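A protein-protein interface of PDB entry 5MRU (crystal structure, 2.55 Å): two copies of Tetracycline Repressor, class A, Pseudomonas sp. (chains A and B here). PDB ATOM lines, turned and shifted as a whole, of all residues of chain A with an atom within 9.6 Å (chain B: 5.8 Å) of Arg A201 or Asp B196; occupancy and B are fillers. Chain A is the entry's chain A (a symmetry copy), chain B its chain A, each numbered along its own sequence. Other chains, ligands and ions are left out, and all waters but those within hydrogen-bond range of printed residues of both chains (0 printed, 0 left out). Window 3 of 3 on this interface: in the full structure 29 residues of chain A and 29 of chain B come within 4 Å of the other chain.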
ATOM      1  N   TRP A  75     -17.118 -37.462  33.134  1.00  0.00           N
ATOM      2  CA  TRP A  75     -17.093 -36.322  32.192  1.00  0.00           C
ATOM      3  C   TRP A  75     -16.325 -36.623  30.886  1.00  0.00           C
ATOM      4  O   TRP A  75     -16.874 -36.437  29.815  1.00  0.00           O
ATOM      5  CB  TRP A  75     -16.665 -34.999  32.880  1.00  0.00           C
ATOM      6  CG  TRP A  75     -15.215 -34.812  33.191  1.00  0.00           C
ATOM      7  CD1 TRP A  75     -14.602 -35.064  34.365  1.00  0.00           C
ATOM      8  CD2 TRP A  75     -14.213 -34.278  32.322  1.00  0.00           C
ATOM      9  NE1 TRP A  75     -13.269 -34.740  34.290  1.00  0.00           N
ATOM     10  CE2 TRP A  75     -13.007 -34.262  33.037  1.00  0.00           C
ATOM     11  CE3 TRP A  75     -14.214 -33.835  31.002  1.00  0.00           C
ATOM     12  CZ2 TRP A  75     -11.821 -33.808  32.481  1.00  0.00           C
ATOM     13  CZ3 TRP A  75     -13.039 -33.398  30.451  1.00  0.00           C
ATOM     14  CH2 TRP A  75     -11.862 -33.386  31.181  1.00  0.00           C
ATOM     15  N   ARG A  76     -15.098 -37.132  30.982  1.00  0.00           N
ATOM     16  CA  ARG A  76     -14.324 -37.531  29.803  1.00  0.00           C
ATOM     17  C   ARG A  76     -15.141 -38.443  28.914  1.00  0.00           C
ATOM     18  O   ARG A  76     -15.299 -38.167  27.739  1.00  0.00           O
ATOM     19  CB  ARG A  76     -13.041 -38.274  30.184  1.00  0.00           C
ATOM     20  CG  ARG A  76     -11.823 -37.387  30.378  1.00  0.00           C
ATOM     21  CD  ARG A  76     -10.657 -38.195  30.933  1.00  0.00           C
ATOM     22  NE  ARG A  76      -9.689 -37.348  31.625  1.00  0.00           N
ATOM     23  CZ  ARG A  76      -8.776 -36.582  31.027  1.00  0.00           C
ATOM     24  NH1 ARG A  76      -8.699 -36.550  29.696  1.00  0.00           N
ATOM     25  NH2 ARG A  76      -7.938 -35.838  31.764  1.00  0.00           N
ATOM     26  N   LEU A 120     -21.895 -31.393  33.587  1.00  0.00           N
ATOM     27  CA  LEU A 120     -20.507 -30.946  33.551  1.00  0.00           C
ATOM     28  C   LEU A 120     -20.199 -30.021  34.723  1.00  0.00           C
ATOM     29  O   LEU A 120     -19.131 -30.117  35.349  1.00  0.00           O
ATOM     30  CB  LEU A 120     -20.196 -30.261  32.239  1.00  0.00           C
ATOM     31  CG  LEU A 120     -20.313 -31.138  30.962  1.00  0.00           C
ATOM     32  CD1 LEU A 120     -20.543 -30.271  29.735  1.00  0.00           C
ATOM     33  CD2 LEU A 120     -19.109 -32.043  30.725  1.00  0.00           C
ATOM     34  N   CYS A 121     -21.141 -29.143  35.051  1.00  0.00           N
ATOM     35  CA  CYS A 121     -21.021 -28.350  36.274  1.00  0.00           C
ATOM     36  C   CYS A 121     -20.936 -29.260  37.486  1.00  0.00           C
ATOM     37  O   CYS A 121     -20.062 -29.095  38.329  1.00  0.00           O
ATOM     38  CB  CYS A 121     -22.180 -27.370  36.397  1.00  0.00           C
ATOM     39  SG  CYS A 121     -22.156 -26.166  35.052  1.00  0.00           S
ATOM     40  N   ALA A 123     -19.645 -31.989  37.621  1.00  0.00           N
ATOM     41  CA  ALA A 123     -18.335 -32.646  37.604  1.00  0.00           C
ATOM     42  C   ALA A 123     -17.105 -31.741  37.820  1.00  0.00           C
ATOM     43  O   ALA A 123     -15.995 -32.258  38.000  1.00  0.00           O
ATOM     44  CB  ALA A 123     -18.177 -33.442  36.324  1.00  0.00           C
ATOM     45  N   GLY A 124     -17.283 -30.418  37.796  1.00  0.00           N
ATOM     46  CA  GLY A 124     -16.210 -29.486  38.221  1.00  0.00           C
ATOM     47  C   GLY A 124     -15.793 -28.376  37.262  1.00  0.00           C
ATOM     48  O   GLY A 124     -14.804 -27.675  37.506  1.00  0.00           O
ATOM     49  N   PHE A 125     -16.533 -28.216  36.170  1.00  0.00           N
ATOM     50  CA  PHE A 125     -16.309 -27.104  35.249  1.00  0.00           C
ATOM     51  C   PHE A 125     -17.133 -25.875  35.625  1.00  0.00           C
ATOM     52  O   PHE A 125     -18.260 -26.013  36.088  1.00  0.00           O
ATOM     53  CB  PHE A 125     -16.686 -27.537  33.840  1.00  0.00           C
ATOM     54  CG  PHE A 125     -15.629 -28.333  33.166  1.00  0.00           C
ATOM     55  CD1 PHE A 125     -14.571 -27.691  32.539  1.00  0.00           C
ATOM     56  CD2 PHE A 125     -15.678 -29.720  33.161  1.00  0.00           C
ATOM     57  CE1 PHE A 125     -13.580 -28.413  31.914  1.00  0.00           C
ATOM     58  CE2 PHE A 125     -14.691 -30.457  32.530  1.00  0.00           C
ATOM     59  CZ  PHE A 125     -13.638 -29.799  31.906  1.00  0.00           C
ATOM     60  N   SER A 126     -16.595 -24.678  35.399  1.00  0.00           N
ATOM     61  CA  SER A 126     -17.388 -23.451  35.572  1.00  0.00           C
ATOM     62  C   SER A 126     -18.422 -23.302  34.442  1.00  0.00           C
ATOM     63  O   SER A 126     -18.412 -24.054  33.470  1.00  0.00           O
ATOM     64  CB  SER A 126     -16.488 -22.224  35.620  1.00  0.00           C
ATOM     65  OG  SER A 126     -15.970 -21.958  34.332  1.00  0.00           O
ATOM     66  N   ALA A 127     -19.310 -22.320  34.575  1.00  0.00           N
ATOM     67  CA  ALA A 127     -20.401 -22.140  33.614  1.00  0.00           C
ATOM     68  C   ALA A 127     -19.883 -21.895  32.194  1.00  0.00           C
ATOM     69  O   ALA A 127     -20.278 -22.578  31.253  1.00  0.00           O
ATOM     70  CB  ALA A 127     -21.302 -20.994  34.048  1.00  0.00           C
ATOM     71  N   GLY A 128     -18.993 -20.917  32.064  1.00  0.00           N
ATOM     72  CA  GLY A 128     -18.424 -20.533  30.780  1.00  0.00           C
ATOM     73  C   GLY A 128     -17.526 -21.607  30.205  1.00  0.00           C
ATOM     74  O   GLY A 128     -17.430 -21.749  28.985  1.00  0.00           O
ATOM     75  N   ASP A 129     -16.862 -22.354  31.083  1.00  0.00           N
ATOM     76  CA  ASP A 129     -16.067 -23.496  30.660  1.00  0.00           C
ATOM     77  C   ASP A 129     -16.929 -24.586  30.071  1.00  0.00           C
ATOM     78  O   ASP A 129     -16.537 -25.228  29.094  1.00  0.00           O
ATOM     79  CB  ASP A 129     -15.274 -24.088  31.829  1.00  0.00           C
ATOM     80  CG  ASP A 129     -14.067 -23.272  32.181  1.00  0.00           C
ATOM     81  OD1 ASP A 129     -13.517 -22.639  31.259  1.00  0.00           O
ATOM     82  OD2 ASP A 129     -13.659 -23.271  33.370  1.00  0.00           O
ATOM     83  N   ALA A 130     -18.089 -24.819  30.665  1.00  0.00           N
ATOM     84  CA  ALA A 130     -18.957 -25.895  30.185  1.00  0.00           C
ATOM     85  C   ALA A 130     -19.539 -25.571  28.808  1.00  0.00           C
ATOM     86  O   ALA A 130     -19.577 -26.442  27.948  1.00  0.00           O
ATOM     87  CB  ALA A 130     -20.067 -26.194  31.187  1.00  0.00           C
ATOM     88  N   VAL A 131     -19.974 -24.325  28.604  1.00  0.00           N
ATOM     89  CA  VAL A 131     -20.469 -23.883  27.305  1.00  0.00           C
ATOM     90  C   VAL A 131     -19.361 -24.072  26.296  1.00  0.00           C
ATOM     91  O   VAL A 131     -19.598 -24.626  25.214  1.00  0.00           O
ATOM     92  CB  VAL A 131     -20.872 -22.392  27.263  1.00  0.00           C
ATOM     93  CG1 VAL A 131     -21.570 -22.092  25.940  1.00  0.00           C
ATOM     94  CG2 VAL A 131     -21.746 -22.006  28.449  1.00  0.00           C
ATOM     95  N   ASN A 132     -18.160 -23.623  26.665  1.00  0.00           N
ATOM     96  CA  ASN A 132     -16.975 -23.730  25.805  1.00  0.00           C
ATOM     97  C   ASN A 132     -16.588 -25.155  25.420  1.00  0.00           C
ATOM     98  O   ASN A 132     -16.204 -25.399  24.286  1.00  0.00           O
ATOM     99  CB  ASN A 132     -15.751 -23.049  26.431  1.00  0.00           C
ATOM    100  CG  ASN A 132     -14.548 -23.031  25.484  1.00  0.00           C
ATOM    101  OD1 ASN A 132     -13.540 -23.704  25.709  1.00  0.00           O
ATOM    102  ND2 ASN A 132     -14.676 -22.282  24.399  1.00  0.00           N
ATOM    103  N   ALA A 133     -16.686 -26.080  26.362  1.00  0.00           N
ATOM    104  CA  ALA A 133     -16.449 -27.495  26.065  1.00  0.00           C
ATOM    105  C   ALA A 133     -17.437 -28.061  25.017  1.00  0.00           C
ATOM    106  O   ALA A 133     -17.077 -28.916  24.216  1.00  0.00           O
ATOM    107  CB  ALA A 133     -16.498 -28.333  27.345  1.00  0.00           C
ATOM    108  N   THR A 136     -16.922 -26.000  21.512  1.00  0.00           N
ATOM    109  CA  THR A 136     -15.657 -26.285  20.869  1.00  0.00           C
ATOM    110  C   THR A 136     -15.628 -27.677  20.221  1.00  0.00           C
ATOM    111  O   THR A 136     -15.156 -27.853  19.104  1.00  0.00           O
ATOM    112  CB  THR A 136     -14.533 -26.124  21.892  1.00  0.00           C
ATOM    113  OG1 THR A 136     -14.398 -24.731  22.236  1.00  0.00           O
ATOM    114  CG2 THR A 136     -13.233 -26.645  21.345  1.00  0.00           C
ATOM    115  N   ALA A 192      -9.086 -36.032  21.254  1.00  0.00           N
ATOM    116  CA  ALA A 192      -8.209 -36.378  22.408  1.00  0.00           C
ATOM    117  C   ALA A 192      -7.500 -35.134  22.942  1.00  0.00           C
ATOM    118  O   ALA A 192      -7.540 -34.846  24.139  1.00  0.00           O
ATOM    119  CB  ALA A 192      -7.195 -37.444  22.033  1.00  0.00           C
ATOM    120  N   VAL A 193      -6.881 -34.380  22.039  1.00  0.00           N
ATOM    121  CA  VAL A 193      -6.267 -33.101  22.382  1.00  0.00           C
ATOM    122  C   VAL A 193      -7.285 -32.163  23.034  1.00  0.00           C
ATOM    123  O   VAL A 193      -7.023 -31.513  24.047  1.00  0.00           O
ATOM    124  CB  VAL A 193      -5.717 -32.429  21.129  1.00  0.00           C
ATOM    125  CG1 VAL A 193      -5.230 -31.025  21.454  1.00  0.00           C
ATOM    126  CG2 VAL A 193      -4.621 -33.278  20.521  1.00  0.00           C
ATOM    127  N   ILE A 194      -8.460 -32.091  22.454  1.00  0.00           N
ATOM    128  CA  ILE A 194      -9.467 -31.218  23.016  1.00  0.00           C
ATOM    129  C   ILE A 194      -9.818 -31.613  24.437  1.00  0.00           C
ATOM    130  O   ILE A 194      -9.996 -30.759  25.285  1.00  0.00           O
ATOM    131  CB  ILE A 194     -10.721 -31.160  22.120  1.00  0.00           C
ATOM    132  CG1 ILE A 194     -10.504 -30.090  21.032  1.00  0.00           C
ATOM    133  CG2 ILE A 194     -11.990 -30.890  22.940  1.00  0.00           C
ATOM    134  CD1 ILE A 194     -11.479 -30.169  19.869  1.00  0.00           C
ATOM    135  N   VAL A 195      -9.915 -32.896  24.710  1.00  0.00           N
ATOM    136  CA  VAL A 195     -10.381 -33.299  26.015  1.00  0.00           C
ATOM    137  C   VAL A 195      -9.310 -32.995  27.072  1.00  0.00           C
ATOM    138  O   VAL A 195      -9.622 -32.728  28.251  1.00  0.00           O
ATOM    139  CB  VAL A 195     -10.794 -34.785  26.035  1.00  0.00           C
ATOM    140  CG1 VAL A 195      -9.719 -35.679  26.664  1.00  0.00           C
ATOM    141  CG2 VAL A 195     -12.108 -34.943  26.777  1.00  0.00           C
ATOM    142  N   ASP A 196      -8.047 -33.041  26.641  1.00  0.00           N
ATOM    143  CA  ASP A 196      -6.931 -32.749  27.537  1.00  0.00           C
ATOM    144  C   ASP A 196      -7.005 -31.273  27.981  1.00  0.00           C
ATOM    145  O   ASP A 196      -7.076 -30.975  29.179  1.00  0.00           O
ATOM    146  CB  ASP A 196      -5.577 -33.063  26.870  1.00  0.00           C
ATOM    147  CG  ASP A 196      -5.338 -34.569  26.657  1.00  0.00           C
ATOM    148  OD1 ASP A 196      -6.252 -35.386  26.879  1.00  0.00           O
ATOM    149  OD2 ASP A 196      -4.221 -34.931  26.252  1.00  0.00           O
ATOM    150  N   GLY A 197      -7.033 -30.357  27.017  1.00  0.00           N
ATOM    151  CA  GLY A 197      -7.064 -28.928  27.326  1.00  0.00           C
ATOM    152  C   GLY A 197      -8.219 -28.502  28.215  1.00  0.00           C
ATOM    153  O   GLY A 197      -8.121 -27.503  28.912  1.00  0.00           O
ATOM    154  N   LEU A 198      -9.322 -29.242  28.177  1.00  0.00           N
ATOM    155  CA  LEU A 198     -10.427 -28.998  29.099  1.00  0.00           C
ATOM    156  C   LEU A 198     -10.097 -29.492  30.496  1.00  0.00           C
ATOM    157  O   LEU A 198     -10.463 -28.846  31.480  1.00  0.00           O
ATOM    158  CB  LEU A 198     -11.685 -29.709  28.632  1.00  0.00           C
ATOM    159  CG  LEU A 198     -12.234 -29.221  27.298  1.00  0.00           C
ATOM    160  CD1 LEU A 198     -13.163 -30.289  26.746  1.00  0.00           C
ATOM    161  CD2 LEU A 198     -12.940 -27.879  27.446  1.00  0.00           C
ATOM    162  N   ALA A 199      -9.430 -30.653  30.582  1.00  0.00           N
ATOM    163  CA  ALA A 199      -8.968 -31.218  31.872  1.00  0.00           C
ATOM    164  C   ALA A 199      -8.143 -30.217  32.671  1.00  0.00           C
ATOM    165  O   ALA A 199      -8.180 -30.241  33.901  1.00  0.00           O
ATOM    166  CB  ALA A 199      -8.186 -32.514  31.665  1.00  0.00           C
ATOM    167  N   LYS A 200      -7.434 -29.325  31.974  1.00  0.00           N
ATOM    168  CA  LYS A 200      -6.775 -28.187  32.626  1.00  0.00           C
ATOM    169  C   LYS A 200      -7.721 -27.224  33.379  1.00  0.00           C
ATOM    170  O   LYS A 200      -7.275 -26.176  33.830  1.00  0.00           O
ATOM    171  CB  LYS A 200      -5.921 -27.391  31.622  1.00  0.00           C
ATOM    172  N   ARG A 201      -9.007 -27.545  33.515  1.00  0.00           N
ATOM    173  CA  ARG A 201      -9.889 -26.750  34.393  1.00  0.00           C
ATOM    174  C   ARG A 201     -11.108 -27.499  34.984  1.00  0.00           C
ATOM    175  O   ARG A 201     -12.075 -26.859  35.443  1.00  0.00           O
ATOM    176  CB  ARG A 201     -10.323 -25.474  33.660  1.00  0.00           C
ATOM    177  CG  ARG A 201     -11.053 -25.716  32.347  1.00  0.00           C
ATOM    178  CD  ARG A 201     -10.837 -24.592  31.339  1.00  0.00           C
ATOM    179  NE  ARG A 201      -9.672 -24.824  30.475  1.00  0.00           N
ATOM    180  CZ  ARG A 201      -9.378 -24.119  29.376  1.00  0.00           C
ATOM    181  NH1 ARG A 201      -8.291 -24.430  28.669  1.00  0.00           N
ATOM    182  NH2 ARG A 201     -10.154 -23.108  28.974  1.00  0.00           N
ATOM    183  N   ARG A 202     -11.038 -28.841  34.987  1.00  0.00           N
ATOM    184  CA  ARG A 202     -11.989 -29.693  35.707  1.00  0.00           C
ATOM    185  C   ARG A 202     -11.805 -29.539  37.231  1.00  0.00           C
ATOM    186  O   ARG A 202     -11.478 -28.459  37.753  1.00  0.00           O
ATOM    187  CB  ARG A 202     -11.808 -31.165  35.306  1.00  0.00           C
ATOM    188  N   TRP B  75       6.079 -21.509  19.389  1.00  0.00           N
ATOM    189  CA  TRP B  75       5.048 -22.437  18.878  1.00  0.00           C
ATOM    190  C   TRP B  75       3.606 -21.994  19.211  1.00  0.00           C
ATOM    191  O   TRP B  75       2.790 -21.894  18.312  1.00  0.00           O
ATOM    192  CB  TRP B  75       5.350 -23.914  19.244  1.00  0.00           C
ATOM    193  CG  TRP B  75       5.089 -24.351  20.650  1.00  0.00           C
ATOM    194  CD1 TRP B  75       5.986 -24.416  21.656  1.00  0.00           C
ATOM    195  CD2 TRP B  75       3.854 -24.835  21.183  1.00  0.00           C
ATOM    196  NE1 TRP B  75       5.392 -24.896  22.798  1.00  0.00           N
ATOM    197  CE2 TRP B  75       4.078 -25.152  22.530  1.00  0.00           C
ATOM    198  CE3 TRP B  75       2.577 -25.010  20.657  1.00  0.00           C
ATOM    199  CZ2 TRP B  75       3.075 -25.645  23.352  1.00  0.00           C
ATOM    200  CZ3 TRP B  75       1.586 -25.485  21.473  1.00  0.00           C
ATOM    201  CH2 TRP B  75       1.834 -25.797  22.800  1.00  0.00           C
ATOM    202  N   ARG B  76       3.321 -21.684  20.474  1.00  0.00           N
ATOM    203  CA  ARG B  76       2.007 -21.171  20.873  1.00  0.00           C
ATOM    204  C   ARG B  76       1.604 -20.003  20.001  1.00  0.00           C
ATOM    205  O   ARG B  76       0.539 -20.022  19.411  1.00  0.00           O
ATOM    206  CB  ARG B  76       1.995 -20.696  22.329  1.00  0.00           C
ATOM    207  CG  ARG B  76       1.616 -21.759  23.345  1.00  0.00           C
ATOM    208  CD  ARG B  76       1.816 -21.237  24.762  1.00  0.00           C
ATOM    209  NE  ARG B  76       1.992 -22.325  25.722  1.00  0.00           N
ATOM    210  CZ  ARG B  76       1.007 -23.076  26.217  1.00  0.00           C
ATOM    211  NH1 ARG B  76      -0.253 -22.859  25.839  1.00  0.00           N
ATOM    212  NH2 ARG B  76       1.285 -24.054  27.091  1.00  0.00           N
ATOM    213  N   GLN B 189     -11.697 -18.897  22.617  1.00  0.00           N
ATOM    214  CA  GLN B 189     -11.698 -19.879  23.701  1.00  0.00           C
ATOM    215  C   GLN B 189     -11.393 -21.295  23.222  1.00  0.00           C
ATOM    216  O   GLN B 189     -10.506 -21.945  23.767  1.00  0.00           O
ATOM    217  CB  GLN B 189     -13.038 -19.912  24.439  1.00  0.00           C
ATOM    218  CG  GLN B 189     -13.194 -18.910  25.571  1.00  0.00           C
ATOM    219  CD  GLN B 189     -14.557 -19.007  26.245  1.00  0.00           C
ATOM    220  OE1 GLN B 189     -15.369 -19.891  25.942  1.00  0.00           O
ATOM    221  NE2 GLN B 189     -14.819 -18.095  27.164  1.00  0.00           N
ATOM    222  N   LEU B 191      -9.942 -22.385  20.732  1.00  0.00           N
ATOM    223  CA  LEU B 191      -8.557 -22.361  20.294  1.00  0.00           C
ATOM    224  C   LEU B 191      -7.608 -22.377  21.490  1.00  0.00           C
ATOM    225  O   LEU B 191      -6.547 -22.992  21.416  1.00  0.00           O
ATOM    226  CB  LEU B 191      -8.304 -21.095  19.477  1.00  0.00           C
ATOM    227  CG  LEU B 191      -6.865 -20.851  19.059  1.00  0.00           C
ATOM    228  CD1 LEU B 191      -6.334 -21.993  18.189  1.00  0.00           C
ATOM    229  CD2 LEU B 191      -6.713 -19.522  18.353  1.00  0.00           C
ATOM    230  N   ALA B 192      -7.975 -21.673  22.574  1.00  0.00           N
ATOM    231  CA  ALA B 192      -7.180 -21.678  23.835  1.00  0.00           C
ATOM    232  C   ALA B 192      -7.109 -23.087  24.426  1.00  0.00           C
ATOM    233  O   ALA B 192      -6.029 -23.593  24.731  1.00  0.00           O
ATOM    234  CB  ALA B 192      -7.749 -20.707  24.853  1.00  0.00           C
ATOM    235  N   VAL B 193      -8.267 -23.727  24.550  1.00  0.00           N
ATOM    236  CA  VAL B 193      -8.344 -25.118  24.983  1.00  0.00           C
ATOM    237  C   VAL B 193      -7.501 -26.020  24.078  1.00  0.00           C
ATOM    238  O   VAL B 193      -6.749 -26.883  24.530  1.00  0.00           O
ATOM    239  CB  VAL B 193      -9.789 -25.603  24.944  1.00  0.00           C
ATOM    240  CG1 VAL B 193      -9.854 -27.095  25.229  1.00  0.00           C
ATOM    241  CG2 VAL B 193     -10.632 -24.807  25.918  1.00  0.00           C
ATOM    242  N   ILE B 194      -7.623 -25.820  22.787  1.00  0.00           N
ATOM    243  CA  ILE B 194      -6.858 -26.642  21.875  1.00  0.00           C
ATOM    244  C   ILE B 194      -5.366 -26.487  22.100  1.00  0.00           C
ATOM    245  O   ILE B 194      -4.634 -27.457  22.052  1.00  0.00           O
ATOM    246  CB  ILE B 194      -7.240 -26.356  20.408  1.00  0.00           C
ATOM    247  CG1 ILE B 194      -8.466 -27.213  20.039  1.00  0.00           C
ATOM    248  CG2 ILE B 194      -6.062 -26.607  19.457  1.00  0.00           C
ATOM    249  CD1 ILE B 194      -9.177 -26.780  18.769  1.00  0.00           C
ATOM    250  N   VAL B 195      -4.907 -25.279  22.350  1.00  0.00           N
ATOM    251  CA  VAL B 195      -3.480 -25.079  22.432  1.00  0.00           C
ATOM    252  C   VAL B 195      -2.933 -25.723  23.713  1.00  0.00           C
ATOM    253  O   VAL B 195      -1.768 -26.169  23.765  1.00  0.00           O
ATOM    254  CB  VAL B 195      -3.114 -23.583  22.346  1.00  0.00           C
ATOM    255  CG1 VAL B 195      -2.801 -22.980  23.721  1.00  0.00           C
ATOM    256  CG2 VAL B 195      -1.933 -23.397  21.410  1.00  0.00           C
ATOM    257  N   ASP B 196      -3.779 -25.765  24.745  1.00  0.00           N
ATOM    258  CA  ASP B 196      -3.394 -26.371  26.016  1.00  0.00           C
ATOM    259  C   ASP B 196      -3.156 -27.883  25.809  1.00  0.00           C
ATOM    260  O   ASP B 196      -2.065 -28.395  26.084  1.00  0.00           O
ATOM    261  CB  ASP B 196      -4.456 -26.120  27.105  1.00  0.00           C
ATOM    262  CG  ASP B 196      -4.536 -24.647  27.547  1.00  0.00           C
ATOM    263  OD1 ASP B 196      -3.892 -23.773  26.935  1.00  0.00           O
ATOM    264  OD2 ASP B 196      -5.265 -24.366  28.513  1.00  0.00           O
ATOM    265  N   GLY B 197      -4.159 -28.582  25.285  1.00  0.00           N
ATOM    266  CA  GLY B 197      -4.054 -30.026  25.082  1.00  0.00           C
ATOM    267  C   GLY B 197      -2.874 -30.457  24.228  1.00  0.00           C
ATOM    268  O   GLY B 197      -2.401 -31.577  24.356  1.00  0.00           O
ATOM    269  N   LEU B 198      -2.412 -29.583  23.341  1.00  0.00           N
ATOM    270  CA  LEU B 198      -1.195 -29.850  22.581  1.00  0.00           C
ATOM    271  C   LEU B 198       0.042 -29.685  23.446  1.00  0.00           C
ATOM    272  O   LEU B 198       0.995 -30.455  23.309  1.00  0.00           O
ATOM    273  CB  LEU B 198      -1.077 -28.900  21.402  1.00  0.00           C
ATOM    274  CG  LEU B 198      -2.176 -29.041  20.358  1.00  0.00           C
ATOM    275  CD1 LEU B 198      -2.207 -27.771  19.524  1.00  0.00           C
ATOM    276  CD2 LEU B 198      -1.964 -30.279  19.495  1.00  0.00           C
ATOM    277  N   ALA B 199       0.036 -28.664  24.316  1.00  0.00           N
ATOM    278  CA  ALA B 199       1.136 -28.427  25.280  1.00  0.00           C
ATOM    279  C   ALA B 199       1.441 -29.665  26.113  1.00  0.00           C
ATOM    280  O   ALA B 199       2.593 -29.876  26.493  1.00  0.00           O
ATOM    281  CB  ALA B 199       0.837 -27.232  26.184  1.00  0.00           C
ATOM    282  N   LYS B 200       0.422 -30.492  26.363  1.00  0.00           N
ATOM    283  CA  LYS B 200       0.633 -31.813  26.967  1.00  0.00           C
ATOM    284  C   LYS B 200       1.540 -32.768  26.157  1.00  0.00           C
ATOM    285  O   LYS B 200       1.655 -33.934  26.516  1.00  0.00           O
ATOM    286  CB  LYS B 200      -0.709 -32.507  27.267  1.00  0.00           C
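The backbone carbonyl oxygen (O) of Asn A132 sits at hydrogen-bond distance from the side-chain hydroxyl (OG1) of Thr A136 (2.8 Å). The guanidinium group of Arg A76 lies within salt-bridge range of the side-chain carboxylate of Asp A196 (3.9 Å). The guanidinium group (NH1) of Arg B76 is in salt-bridge range of the side-chain carboxylate (OD1) of Asp B196. O of Gly A197 sits at hydrogen-bond distance from NH1 of Arg A201 (3.1 Å).
Of the 27 printed residues of chain A, 7 touch a printed residue of chain B. Hydrophobic or aromatic side chains of chain A within 4 Å of the printed part of chain B: Val A193, Ile A194 and Leu A198. Among the printed residues, 14 pairs touch across the chains. Among the printed residues, Asp or Glu carboxylates within 4 Å of a Lys or Arg side-chain nitrogen of the other chain: Arg A201 with Asp B196 (3.0 Å).
NH1 of Arg A201 lies within salt-bridge range of OD2 of Asp B196 (3.0 Å). The side-chain amide oxygen of Gln B189 sits close to the side-chain amide nitrogen of Asn A132, at 2.9 Å.
Val A193 touches Ile B194, and with the chains exchanged Ile A194 touches Val B193. Val A193 touches Leu B198, and with the chains exchanged Leu A198 touches Val B193. Ile B194 touches its own counterpart, Ile A194. Asp A196 touches Gly B197, and with the chains exchanged Gly A197 touches Asp B196. Of the 14 pairs that touch across the chains among the printed residues, 10 have their exchanged pair printed and touching as well.
Among the printed residues, pairs that only touch across the chains: Asn A132 with Val B193, Val A193 with Gly B197, Gly A197 with Val B193, Arg A201 with Val B193, Gly A197 with Gly B197, Ile A194 with Ile B194, Val A193 with Ile B194, Ile A194 with Val B193, Val A193 with Leu B198, Leu A198 with Val B193, Gly A197 with Asp B196 and Asp A196 with Gly B197.
Of the printed residues of chain B, Gly A197 touches Val B193, Asp B196 and Gly B197. Of chain B, only Val B193 (3.5 Å) and Asp B196 (3.0 Å) come within 4 Å of Arg A201. Printed residues of chain A within 4 Å of Gln B189: Asn A132 (2.9 Å). Of chain A, only Asn A132 (3.1 Å), Ile A194 (3.7 Å), Gly A197 (3.5 Å), Leu A198 (3.7 Å) and Arg A201 (3.5 Å) come within 4 Å of Val B193. No residue of chain A comes within 4 Å of Val B195. Asp B196 touches two residues of chain A. Gly B197 touches just these residues of chain A: Val A193, Asp A196 and Gly A197. The nearest residue of chain A that does not touch Asp B196 is Lys A200 (4.4 Å). The nearest printed residue of chain A that does not touch Gln B189 is Gly A128 (4.1 Å).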
